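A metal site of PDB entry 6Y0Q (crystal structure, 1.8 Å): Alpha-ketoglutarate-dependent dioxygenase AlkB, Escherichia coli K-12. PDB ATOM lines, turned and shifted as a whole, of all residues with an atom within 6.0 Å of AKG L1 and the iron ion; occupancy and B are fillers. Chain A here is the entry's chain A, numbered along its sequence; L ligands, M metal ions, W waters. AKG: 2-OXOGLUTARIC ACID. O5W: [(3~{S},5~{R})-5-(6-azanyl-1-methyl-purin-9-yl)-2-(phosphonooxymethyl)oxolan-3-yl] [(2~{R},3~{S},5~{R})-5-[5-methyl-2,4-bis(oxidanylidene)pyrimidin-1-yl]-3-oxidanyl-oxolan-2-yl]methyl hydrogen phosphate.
Leu 118 touches AKG L1 (CD2 to O1, 3.6 Å). Leu 128 touches AKG L1 (CD2 to C2, 3.5 Å). Ile 189 touches AKG L1 (CG1 to O3, 3.6 Å). 11 residues have an atom within 4 Å of AKG L1: Leu 118, Asn 120, Tyr 122, Leu 128, His 131, Asp 133, His 187, Ile 189, Arg 204, Asn 206 and Arg 210. The nearest printed residue that does not touch AKG L1 is Met 61 (4.1 Å).
The side-chain hydroxyl (OH) of Tyr 122 is in hydrogen-bond range of the side-chain amide nitrogen (ND2) of Asn 120 (3.3 Å). The backbone NH (N) of Thr 208 sits at hydrogen-bond distance from the backbone carbonyl oxygen (O) of Leu 118 (2.9 Å). ND2 of Asn 206 sits close to NH2 of Arg 204, at 3.5 Å. The side-chain hydroxyl (OG) of Ser 147 lies within hydrogen-bond range of the guanidinium group (NH2) of Arg 204 (2.8 Å). The backbone NH of Asn 120 lies within hydrogen-bond range of the backbone carbonyl oxygen of Asn 206, at 2.8 Å. ND2 of Asn 206 sits at hydrogen-bond distance from OG of Ser 145 (2.9 Å). The guanidinium group (NH2) of Arg 210 lies within hydrogen-bond range of the side-chain hydroxyl (OG1) of Thr 208. The backbone carbonyl oxygen (O) of Arg 204 lies within hydrogen-bond range of the backbone NH (N) of Tyr 122 (2.8 Å).
Water W1 lies within hydrogen-bond range of O4 of AKG L1 (2.7 Å) and OG of Ser 145 (2.8 Å).
ND2 of Asn 206 sits at hydrogen-bond distance from O4 of AKG L1, at 3.2 Å. The side-chain hydroxyl of Tyr 122 is in hydrogen-bond range of an oxygen (O3) of AKG L1. An oxygen (O3) of AKG L1 lies within salt-bridge range of the guanidinium group (NH1) of Arg 204 (2.8 Å). ND2 of Asn 120 is in hydrogen-bond range of O1 of AKG L1, at 3.0 Å. An oxygen (O2) of AKG L1 lies close to the guanidinium group (NH2) of Arg 210.
O2 of AKG L1 binds the iron ion. The side-chain carboxylate (OD1) of Asp 133 binds the iron ion (2.1 Å). NE2 of His 187 binds the iron ion, 2.1 Å away. NE2 of His 131 is bound to the iron ion (2.2 Å). Water W2 binds the iron ion. An oxygen (O5) of AKG L1 is bound to the iron ion (2.4 Å). The iron ion has six donor atoms within binding distance.
Within 4 Å of the iron ion: His 131, Asp 133 and His 187.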
ATOM      1  N   MET A  61      -7.995  14.463 -17.488  1.00  0.00           N
ATOM      2  CA  MET A  61      -9.195  14.072 -16.765  1.00  0.00           C
ATOM      3  C   MET A  61     -10.074  13.170 -17.613  1.00  0.00           C
ATOM      4  O   MET A  61     -10.060  13.209 -18.852  1.00  0.00           O
ATOM      5  CB  MET A  61     -10.039  15.299 -16.355  1.00  0.00           C
ATOM      6  CG  MET A  61      -9.414  16.166 -15.286  1.00  0.00           C
ATOM      7  SD  MET A  61     -10.282  17.724 -15.122  1.00  0.00           S
ATOM      8  CE  MET A  61      -9.686  18.271 -13.521  1.00  0.00           C
ATOM      9  N   LEU A 118     -14.920  12.012 -10.902  1.00  0.00           N
ATOM     10  CA  LEU A 118     -13.909  12.648 -11.723  1.00  0.00           C
ATOM     11  C   LEU A 118     -12.572  11.972 -11.467  1.00  0.00           C
ATOM     12  O   LEU A 118     -12.186  11.778 -10.310  1.00  0.00           O
ATOM     13  CB  LEU A 118     -13.842  14.137 -11.397  1.00  0.00           C
ATOM     14  CG  LEU A 118     -12.825  14.973 -12.161  1.00  0.00           C
ATOM     15  CD1 LEU A 118     -13.134  14.981 -13.653  1.00  0.00           C
ATOM     16  CD2 LEU A 118     -12.820  16.387 -11.594  1.00  0.00           C
ATOM     17  N   ASN A 120      -8.556  12.267 -12.209  1.00  0.00           N
ATOM     18  CA  ASN A 120      -7.463  13.142 -12.597  1.00  0.00           C
ATOM     19  C   ASN A 120      -6.163  12.350 -12.719  1.00  0.00           C
ATOM     20  O   ASN A 120      -5.851  11.534 -11.849  1.00  0.00           O
ATOM     21  CB  ASN A 120      -7.232  14.254 -11.565  1.00  0.00           C
ATOM     22  CG  ASN A 120      -8.401  15.203 -11.434  1.00  0.00           C
ATOM     23  OD1 ASN A 120      -9.457  15.015 -12.033  1.00  0.00           O
ATOM     24  ND2 ASN A 120      -8.218  16.243 -10.635  1.00  0.00           N
ATOM     25  N   TYR A 122      -2.032  13.085 -13.134  1.00  0.00           N
ATOM     26  CA  TYR A 122      -0.968  14.070 -13.025  1.00  0.00           C
ATOM     27  C   TYR A 122       0.342  13.439 -13.475  1.00  0.00           C
ATOM     28  O   TYR A 122       0.828  12.502 -12.836  1.00  0.00           O
ATOM     29  CB  TYR A 122      -0.810  14.579 -11.588  1.00  0.00           C
ATOM     30  CG  TYR A 122      -2.024  15.265 -11.004  1.00  0.00           C
ATOM     31  CD1 TYR A 122      -3.080  14.530 -10.483  1.00  0.00           C
ATOM     32  CD2 TYR A 122      -2.089  16.638 -10.940  1.00  0.00           C
ATOM     33  CE1 TYR A 122      -4.183  15.159  -9.936  1.00  0.00           C
ATOM     34  CE2 TYR A 122      -3.187  17.275 -10.403  1.00  0.00           C
ATOM     35  CZ  TYR A 122      -4.233  16.528  -9.898  1.00  0.00           C
ATOM     36  OH  TYR A 122      -5.314  17.192  -9.360  1.00  0.00           O
ATOM     37  N   LEU A 128      -2.650  21.894 -10.375  1.00  0.00           N
ATOM     38  CA  LEU A 128      -4.041  22.343 -10.431  1.00  0.00           C
ATOM     39  C   LEU A 128      -4.143  23.573  -9.539  1.00  0.00           C
ATOM     40  O   LEU A 128      -3.963  23.473  -8.326  1.00  0.00           O
ATOM     41  CB  LEU A 128      -4.987  21.239  -9.974  1.00  0.00           C
ATOM     42  CG  LEU A 128      -6.472  21.533 -10.037  1.00  0.00           C
ATOM     43  CD1 LEU A 128      -6.892  21.881 -11.460  1.00  0.00           C
ATOM     44  CD2 LEU A 128      -7.251  20.329  -9.524  1.00  0.00           C
ATOM     45  N   HIS A 131      -8.971  26.625  -6.577  1.00  0.00           N
ATOM     46  CA  HIS A 131     -10.348  26.724  -7.026  1.00  0.00           C
ATOM     47  C   HIS A 131     -11.252  26.189  -5.929  1.00  0.00           C
ATOM     48  O   HIS A 131     -10.813  25.508  -5.001  1.00  0.00           O
ATOM     49  CB  HIS A 131     -10.581  25.901  -8.295  1.00  0.00           C
ATOM     50  CG  HIS A 131     -10.405  24.440  -8.067  1.00  0.00           C
ATOM     51  ND1 HIS A 131      -9.173  23.832  -8.076  1.00  0.00           N
ATOM     52  CD2 HIS A 131     -11.304  23.468  -7.754  1.00  0.00           C
ATOM     53  CE1 HIS A 131      -9.319  22.539  -7.814  1.00  0.00           C
ATOM     54  NE2 HIS A 131     -10.607  22.299  -7.605  1.00  0.00           N
ATOM     55  N   GLN A 132     -12.543  26.496  -6.067  1.00  0.00           N
ATOM     56  CA  GLN A 132     -13.607  25.869  -5.315  1.00  0.00           C
ATOM     57  C   GLN A 132     -14.407  24.931  -6.220  1.00  0.00           C
ATOM     58  O   GLN A 132     -14.505  25.151  -7.430  1.00  0.00           O
ATOM     59  CB  GLN A 132     -14.571  26.899  -4.715  1.00  0.00           C
ATOM     60  CG  GLN A 132     -13.981  27.819  -3.680  1.00  0.00           C
ATOM     61  CD  GLN A 132     -14.976  28.870  -3.236  1.00  0.00           C
ATOM     62  OE1 GLN A 132     -15.495  29.642  -4.045  1.00  0.00           O
ATOM     63  NE2 GLN A 132     -15.261  28.911  -1.939  1.00  0.00           N
ATOM     64  N   ASP A 133     -14.999  23.919  -5.601  1.00  0.00           N
ATOM     65  CA  ASP A 133     -15.907  22.975  -6.262  1.00  0.00           C
ATOM     66  C   ASP A 133     -17.328  23.405  -5.907  1.00  0.00           C
ATOM     67  O   ASP A 133     -17.824  23.100  -4.822  1.00  0.00           O
ATOM     68  CB  ASP A 133     -15.629  21.556  -5.789  1.00  0.00           C
ATOM     69  CG  ASP A 133     -14.407  20.928  -6.469  1.00  0.00           C
ATOM     70  OD1 ASP A 133     -13.311  21.530  -6.418  1.00  0.00           O
ATOM     71  OD2 ASP A 133     -14.560  19.843  -7.054  1.00  0.00           O
ATOM     72  N   SER A 145     -12.221  12.046  -1.799  1.00  0.00           N
ATOM     73  CA  SER A 145     -11.030  12.109  -2.634  1.00  0.00           C
ATOM     74  C   SER A 145     -10.095  10.937  -2.324  1.00  0.00           C
ATOM     75  O   SER A 145      -9.785  10.679  -1.161  1.00  0.00           O
ATOM     76  CB  SER A 145     -10.282  13.420  -2.399  1.00  0.00           C
ATOM     77  OG  SER A 145      -8.965  13.363  -2.931  1.00  0.00           O
ATOM     78  N   SER A 147      -6.337   9.173  -3.432  1.00  0.00           N
ATOM     79  CA  SER A 147      -5.045   9.430  -4.067  1.00  0.00           C
ATOM     80  C   SER A 147      -4.321   8.110  -4.350  1.00  0.00           C
ATOM     81  O   SER A 147      -4.290   7.221  -3.500  1.00  0.00           O
ATOM     82  CB  SER A 147      -4.173  10.328  -3.186  1.00  0.00           C
ATOM     83  OG  SER A 147      -4.684  11.657  -3.108  1.00  0.00           O
ATOM     84  N   PHE A 154      -0.983  18.904  -1.500  1.00  0.00           N
ATOM     85  CA  PHE A 154      -2.310  19.489  -1.598  1.00  0.00           C
ATOM     86  C   PHE A 154      -2.306  20.788  -0.802  1.00  0.00           C
ATOM     87  O   PHE A 154      -1.862  20.805   0.350  1.00  0.00           O
ATOM     88  CB  PHE A 154      -3.341  18.495  -1.048  1.00  0.00           C
ATOM     89  CG  PHE A 154      -4.767  18.969  -1.102  1.00  0.00           C
ATOM     90  CD1 PHE A 154      -5.532  18.760  -2.223  1.00  0.00           C
ATOM     91  CD2 PHE A 154      -5.353  19.596  -0.009  1.00  0.00           C
ATOM     92  CE1 PHE A 154      -6.844  19.177  -2.272  1.00  0.00           C
ATOM     93  CE2 PHE A 154      -6.657  20.019  -0.059  1.00  0.00           C
ATOM     94  CZ  PHE A 154      -7.406  19.807  -1.174  1.00  0.00           C
ATOM     95  N   LEU A 170      -0.280  14.295   0.321  1.00  0.00           N
ATOM     96  CA  LEU A 170      -1.192  13.192   0.070  1.00  0.00           C
ATOM     97  C   LEU A 170      -0.417  12.068  -0.617  1.00  0.00           C
ATOM     98  O   LEU A 170       0.216  12.292  -1.656  1.00  0.00           O
ATOM     99  CB  LEU A 170      -2.381  13.636  -0.777  1.00  0.00           C
ATOM    100  CG  LEU A 170      -3.361  14.598  -0.102  1.00  0.00           C
ATOM    101  CD1 LEU A 170      -4.467  14.979  -1.064  1.00  0.00           C
ATOM    102  CD2 LEU A 170      -3.940  13.973   1.151  1.00  0.00           C
ATOM    103  N   HIS A 187      -8.734  25.218  -3.011  1.00  0.00           N
ATOM    104  CA  HIS A 187      -7.768  24.128  -2.922  1.00  0.00           C
ATOM    105  C   HIS A 187      -7.119  23.883  -4.281  1.00  0.00           C
ATOM    106  O   HIS A 187      -7.640  24.262  -5.330  1.00  0.00           O
ATOM    107  CB  HIS A 187      -8.448  22.854  -2.404  1.00  0.00           C
ATOM    108  CG  HIS A 187      -9.559  22.380  -3.284  1.00  0.00           C
ATOM    109  ND1 HIS A 187     -10.840  22.895  -3.207  1.00  0.00           N
ATOM    110  CD2 HIS A 187      -9.576  21.467  -4.276  1.00  0.00           C
ATOM    111  CE1 HIS A 187     -11.600  22.298  -4.110  1.00  0.00           C
ATOM    112  NE2 HIS A 187     -10.864  21.425  -4.762  1.00  0.00           N
ATOM    113  N   GLY A 188      -5.955  23.238  -4.230  1.00  0.00           N
ATOM    114  CA  GLY A 188      -5.222  22.938  -5.442  1.00  0.00           C
ATOM    115  C   GLY A 188      -4.089  21.978  -5.160  1.00  0.00           C
ATOM    116  O   GLY A 188      -3.912  21.503  -4.027  1.00  0.00           O
ATOM    117  N   ILE A 189      -3.318  21.697  -6.200  1.00  0.00           N
ATOM    118  CA  ILE A 189      -2.204  20.751  -6.172  1.00  0.00           C
ATOM    119  C   ILE A 189      -0.979  21.452  -6.739  1.00  0.00           C
ATOM    120  O   ILE A 189      -1.049  22.104  -7.791  1.00  0.00           O
ATOM    121  CB  ILE A 189      -2.525  19.485  -6.991  1.00  0.00           C
ATOM    122  CG1 ILE A 189      -3.652  18.693  -6.328  1.00  0.00           C
ATOM    123  CG2 ILE A 189      -1.282  18.613  -7.199  1.00  0.00           C
ATOM    124  CD1 ILE A 189      -3.234  17.924  -5.109  1.00  0.00           C
ATOM    125  N   ARG A 204       0.445  10.286 -10.831  1.00  0.00           N
ATOM    126  CA  ARG A 204      -0.518  10.257  -9.740  1.00  0.00           C
ATOM    127  C   ARG A 204      -1.921  10.250 -10.317  1.00  0.00           C
ATOM    128  O   ARG A 204      -2.203  10.976 -11.274  1.00  0.00           O
ATOM    129  CB  ARG A 204      -0.364  11.482  -8.816  1.00  0.00           C
ATOM    130  CG  ARG A 204      -1.432  11.591  -7.748  1.00  0.00           C
ATOM    131  CD  ARG A 204      -1.215  12.830  -6.867  1.00  0.00           C
ATOM    132  NE  ARG A 204      -2.238  12.960  -5.827  1.00  0.00           N
ATOM    133  CZ  ARG A 204      -3.276  13.799  -5.872  1.00  0.00           C
ATOM    134  NH1 ARG A 204      -3.461  14.620  -6.907  1.00  0.00           N
ATOM    135  NH2 ARG A 204      -4.140  13.830  -4.867  1.00  0.00           N
ATOM    136  N   ASN A 206      -5.986  10.824  -9.035  1.00  0.00           N
ATOM    137  CA  ASN A 206      -6.897  11.227  -7.981  1.00  0.00           C
ATOM    138  C   ASN A 206      -8.319  10.989  -8.451  1.00  0.00           C
ATOM    139  O   ASN A 206      -8.671  11.346  -9.575  1.00  0.00           O
ATOM    140  CB  ASN A 206      -6.700  12.693  -7.596  1.00  0.00           C
ATOM    141  CG  ASN A 206      -7.689  13.171  -6.551  1.00  0.00           C
ATOM    142  OD1 ASN A 206      -8.651  13.864  -6.861  1.00  0.00           O
ATOM    143  ND2 ASN A 206      -7.446  12.798  -5.300  1.00  0.00           N
ATOM    144  N   THR A 208     -12.294  11.825  -7.381  1.00  0.00           N
ATOM    145  CA  THR A 208     -13.189  12.595  -6.513  1.00  0.00           C
ATOM    146  C   THR A 208     -14.631  12.210  -6.817  1.00  0.00           C
ATOM    147  O   THR A 208     -15.126  12.459  -7.927  1.00  0.00           O
ATOM    148  CB  THR A 208     -12.985  14.113  -6.642  1.00  0.00           C
ATOM    149  OG1 THR A 208     -12.928  14.507  -8.013  1.00  0.00           O
ATOM    150  CG2 THR A 208     -11.720  14.545  -5.921  1.00  0.00           C
ATOM    151  N   ARG A 210     -18.626  12.564  -6.324  1.00  0.00           N
ATOM    152  CA  ARG A 210     -19.515  13.697  -6.151  1.00  0.00           C
ATOM    153  C   ARG A 210     -20.977  13.276  -6.259  1.00  0.00           C
ATOM    154  O   ARG A 210     -21.315  12.335  -6.982  1.00  0.00           O
ATOM    155  CB  ARG A 210     -19.208  14.773  -7.193  1.00  0.00           C
ATOM    156  CG  ARG A 210     -17.753  15.228  -7.150  1.00  0.00           C
ATOM    157  CD  ARG A 210     -17.067  15.188  -8.512  1.00  0.00           C
ATOM    158  NE  ARG A 210     -15.670  15.627  -8.375  1.00  0.00           N
ATOM    159  CZ  ARG A 210     -15.307  16.893  -8.171  1.00  0.00           C
ATOM    160  NH1 ARG A 210     -16.219  17.857  -8.098  1.00  0.00           N
ATOM    161  NH2 ARG A 210     -14.019  17.198  -8.023  1.00  0.00           N
HETATM  162  C1  AKG L   1     -10.470  18.654  -8.436  1.00  0.00           C
HETATM  163  O1  AKG L   1     -10.320  18.017  -9.511  1.00  0.00           O
HETATM  164  O2  AKG L   1     -11.491  19.369  -8.258  1.00  0.00           O
HETATM  165  C2  AKG L   1      -9.400  18.560  -7.349  1.00  0.00           C
HETATM  166  O5  AKG L   1      -9.372  19.369  -6.484  1.00  0.00           O
HETATM  167  C3  AKG L   1      -8.351  17.435  -7.412  1.00  0.00           C
HETATM  168  C4  AKG L   1      -7.583  17.394  -6.088  1.00  0.00           C
HETATM  169  C5  AKG L   1      -6.502  16.298  -6.090  1.00  0.00           C
HETATM  170  O3  AKG L   1      -5.900  15.997  -7.156  1.00  0.00           O
HETATM  171  O4  AKG L   1      -6.212  15.730  -5.001  1.00  0.00           O
HETATM  172  C31 O5W L   2      -2.312  29.873 -16.284  1.00  0.00           C
HETATM  173  C32 O5W L   2      -2.143  31.357 -16.223  1.00  0.00           C
HETATM  174  C01 O5W L   2     -13.819  19.724 -10.209  1.00  0.00           C
HETATM  175  C03 O5W L   2     -13.581  22.111 -10.570  1.00  0.00           C
HETATM  176  C04 O5W L   2     -12.793  23.220 -10.988  1.00  0.00           C
HETATM  177  C05 O5W L   2     -11.523  22.979 -11.419  1.00  0.00           C
HETATM  178  C07 O5W L   2     -11.888  25.139 -11.554  1.00  0.00           C
HETATM  179  C09 O5W L   2      -9.622  24.315 -12.246  1.00  0.00           C
HETATM  180  C10 O5W L   2      -9.561  25.058 -13.647  1.00  0.00           C
HETATM  181  C11 O5W L   2      -8.184  25.783 -13.525  1.00  0.00           C
HETATM  182  C12 O5W L   2      -8.067  26.136 -12.264  1.00  0.00           C
HETATM  183  C14 O5W L   2      -8.565  27.513 -12.002  1.00  0.00           C
HETATM  184  C24 O5W L   2      -4.902  25.988 -16.554  1.00  0.00           C
HETATM  185  C25 O5W L   2      -3.406  26.187 -16.882  1.00  0.00           C
HETATM  186  C26 O5W L   2      -2.543  26.454 -15.564  1.00  0.00           C
HETATM  187  C27 O5W L   2      -1.285  27.100 -16.128  1.00  0.00           C
HETATM  188  C28 O5W L   2      -1.660  27.668 -17.291  1.00  0.00           C
HETATM  189  C33 O5W L   2      -1.164  32.038 -17.122  1.00  0.00           C
HETATM  190  C35 O5W L   2      -0.537  29.771 -18.124  1.00  0.00           C
HETATM  191  C38 O5W L   2      -2.980  32.194 -15.231  1.00  0.00           C
HETATM  192  C42 O5W L   2     -11.775  20.700 -11.055  1.00  0.00           C
HETATM  193  N02 O5W L   2     -13.020  20.896 -10.628  1.00  0.00           N
HETATM  194  N06 O5W L   2     -10.995  24.169 -11.760  1.00  0.00           N
HETATM  195  N08 O5W L   2     -13.009  24.571 -11.081  1.00  0.00           N
HETATM  196  N30 O5W L   2      -1.517  29.090 -17.225  1.00  0.00           N
HETATM  197  N34 O5W L   2      -0.377  31.249 -18.063  1.00  0.00           N
HETATM  198  N41 O5W L   2     -11.005  21.708 -11.456  1.00  0.00           N
HETATM  199  N43 O5W L   2     -14.933  22.313 -10.107  1.00  0.00           N
HETATM  200  O13 O5W L   2      -8.981  25.049 -11.394  1.00  0.00           O
HETATM  201  O15 O5W L   2      -9.908  27.589 -12.422  1.00  0.00           O
HETATM  202  O17 O5W L   2     -10.855  29.845 -11.617  1.00  0.00           O
HETATM  203  O18 O5W L   2     -11.833  28.903 -13.808  1.00  0.00           O
HETATM  204  O19 O5W L   2      -9.506  29.907 -13.451  1.00  0.00           O
HETATM  205  O20 O5W L   2      -7.126  24.777 -13.850  1.00  0.00           O
HETATM  206  O22 O5W L   2      -4.635  24.871 -13.013  1.00  0.00           O
HETATM  207  O23 O5W L   2      -5.018  24.925 -15.597  1.00  0.00           O
HETATM  208  O29 O5W L   2      -3.237  27.262 -17.546  1.00  0.00           O
HETATM  209  O36 O5W L   2       0.101  29.129 -18.887  1.00  0.00           O
HETATM  210  O37 O5W L   2      -1.037  33.213 -17.078  1.00  0.00           O
HETATM  211  O39 O5W L   2      -2.250  25.296 -14.931  1.00  0.00           O
HETATM  212  O40 O5W L   2      -5.480  26.761 -13.816  1.00  0.00           O
HETATM  213  P16 O5W L   2     -10.535  29.072 -12.820  1.00  0.00           P
HETATM  214  P21 O5W L   2      -5.543  25.321 -14.050  1.00  0.00           P
HETATM  215 FE    FE M   1     -11.443  20.570  -6.613  1.00  0.00          FE
HETATM  216  O   HOH W   1      -7.954  15.939  -2.950  1.00  0.00           O
HETATM  217  O   HOH W   2     -12.201  18.709  -5.392  1.00  0.00           O
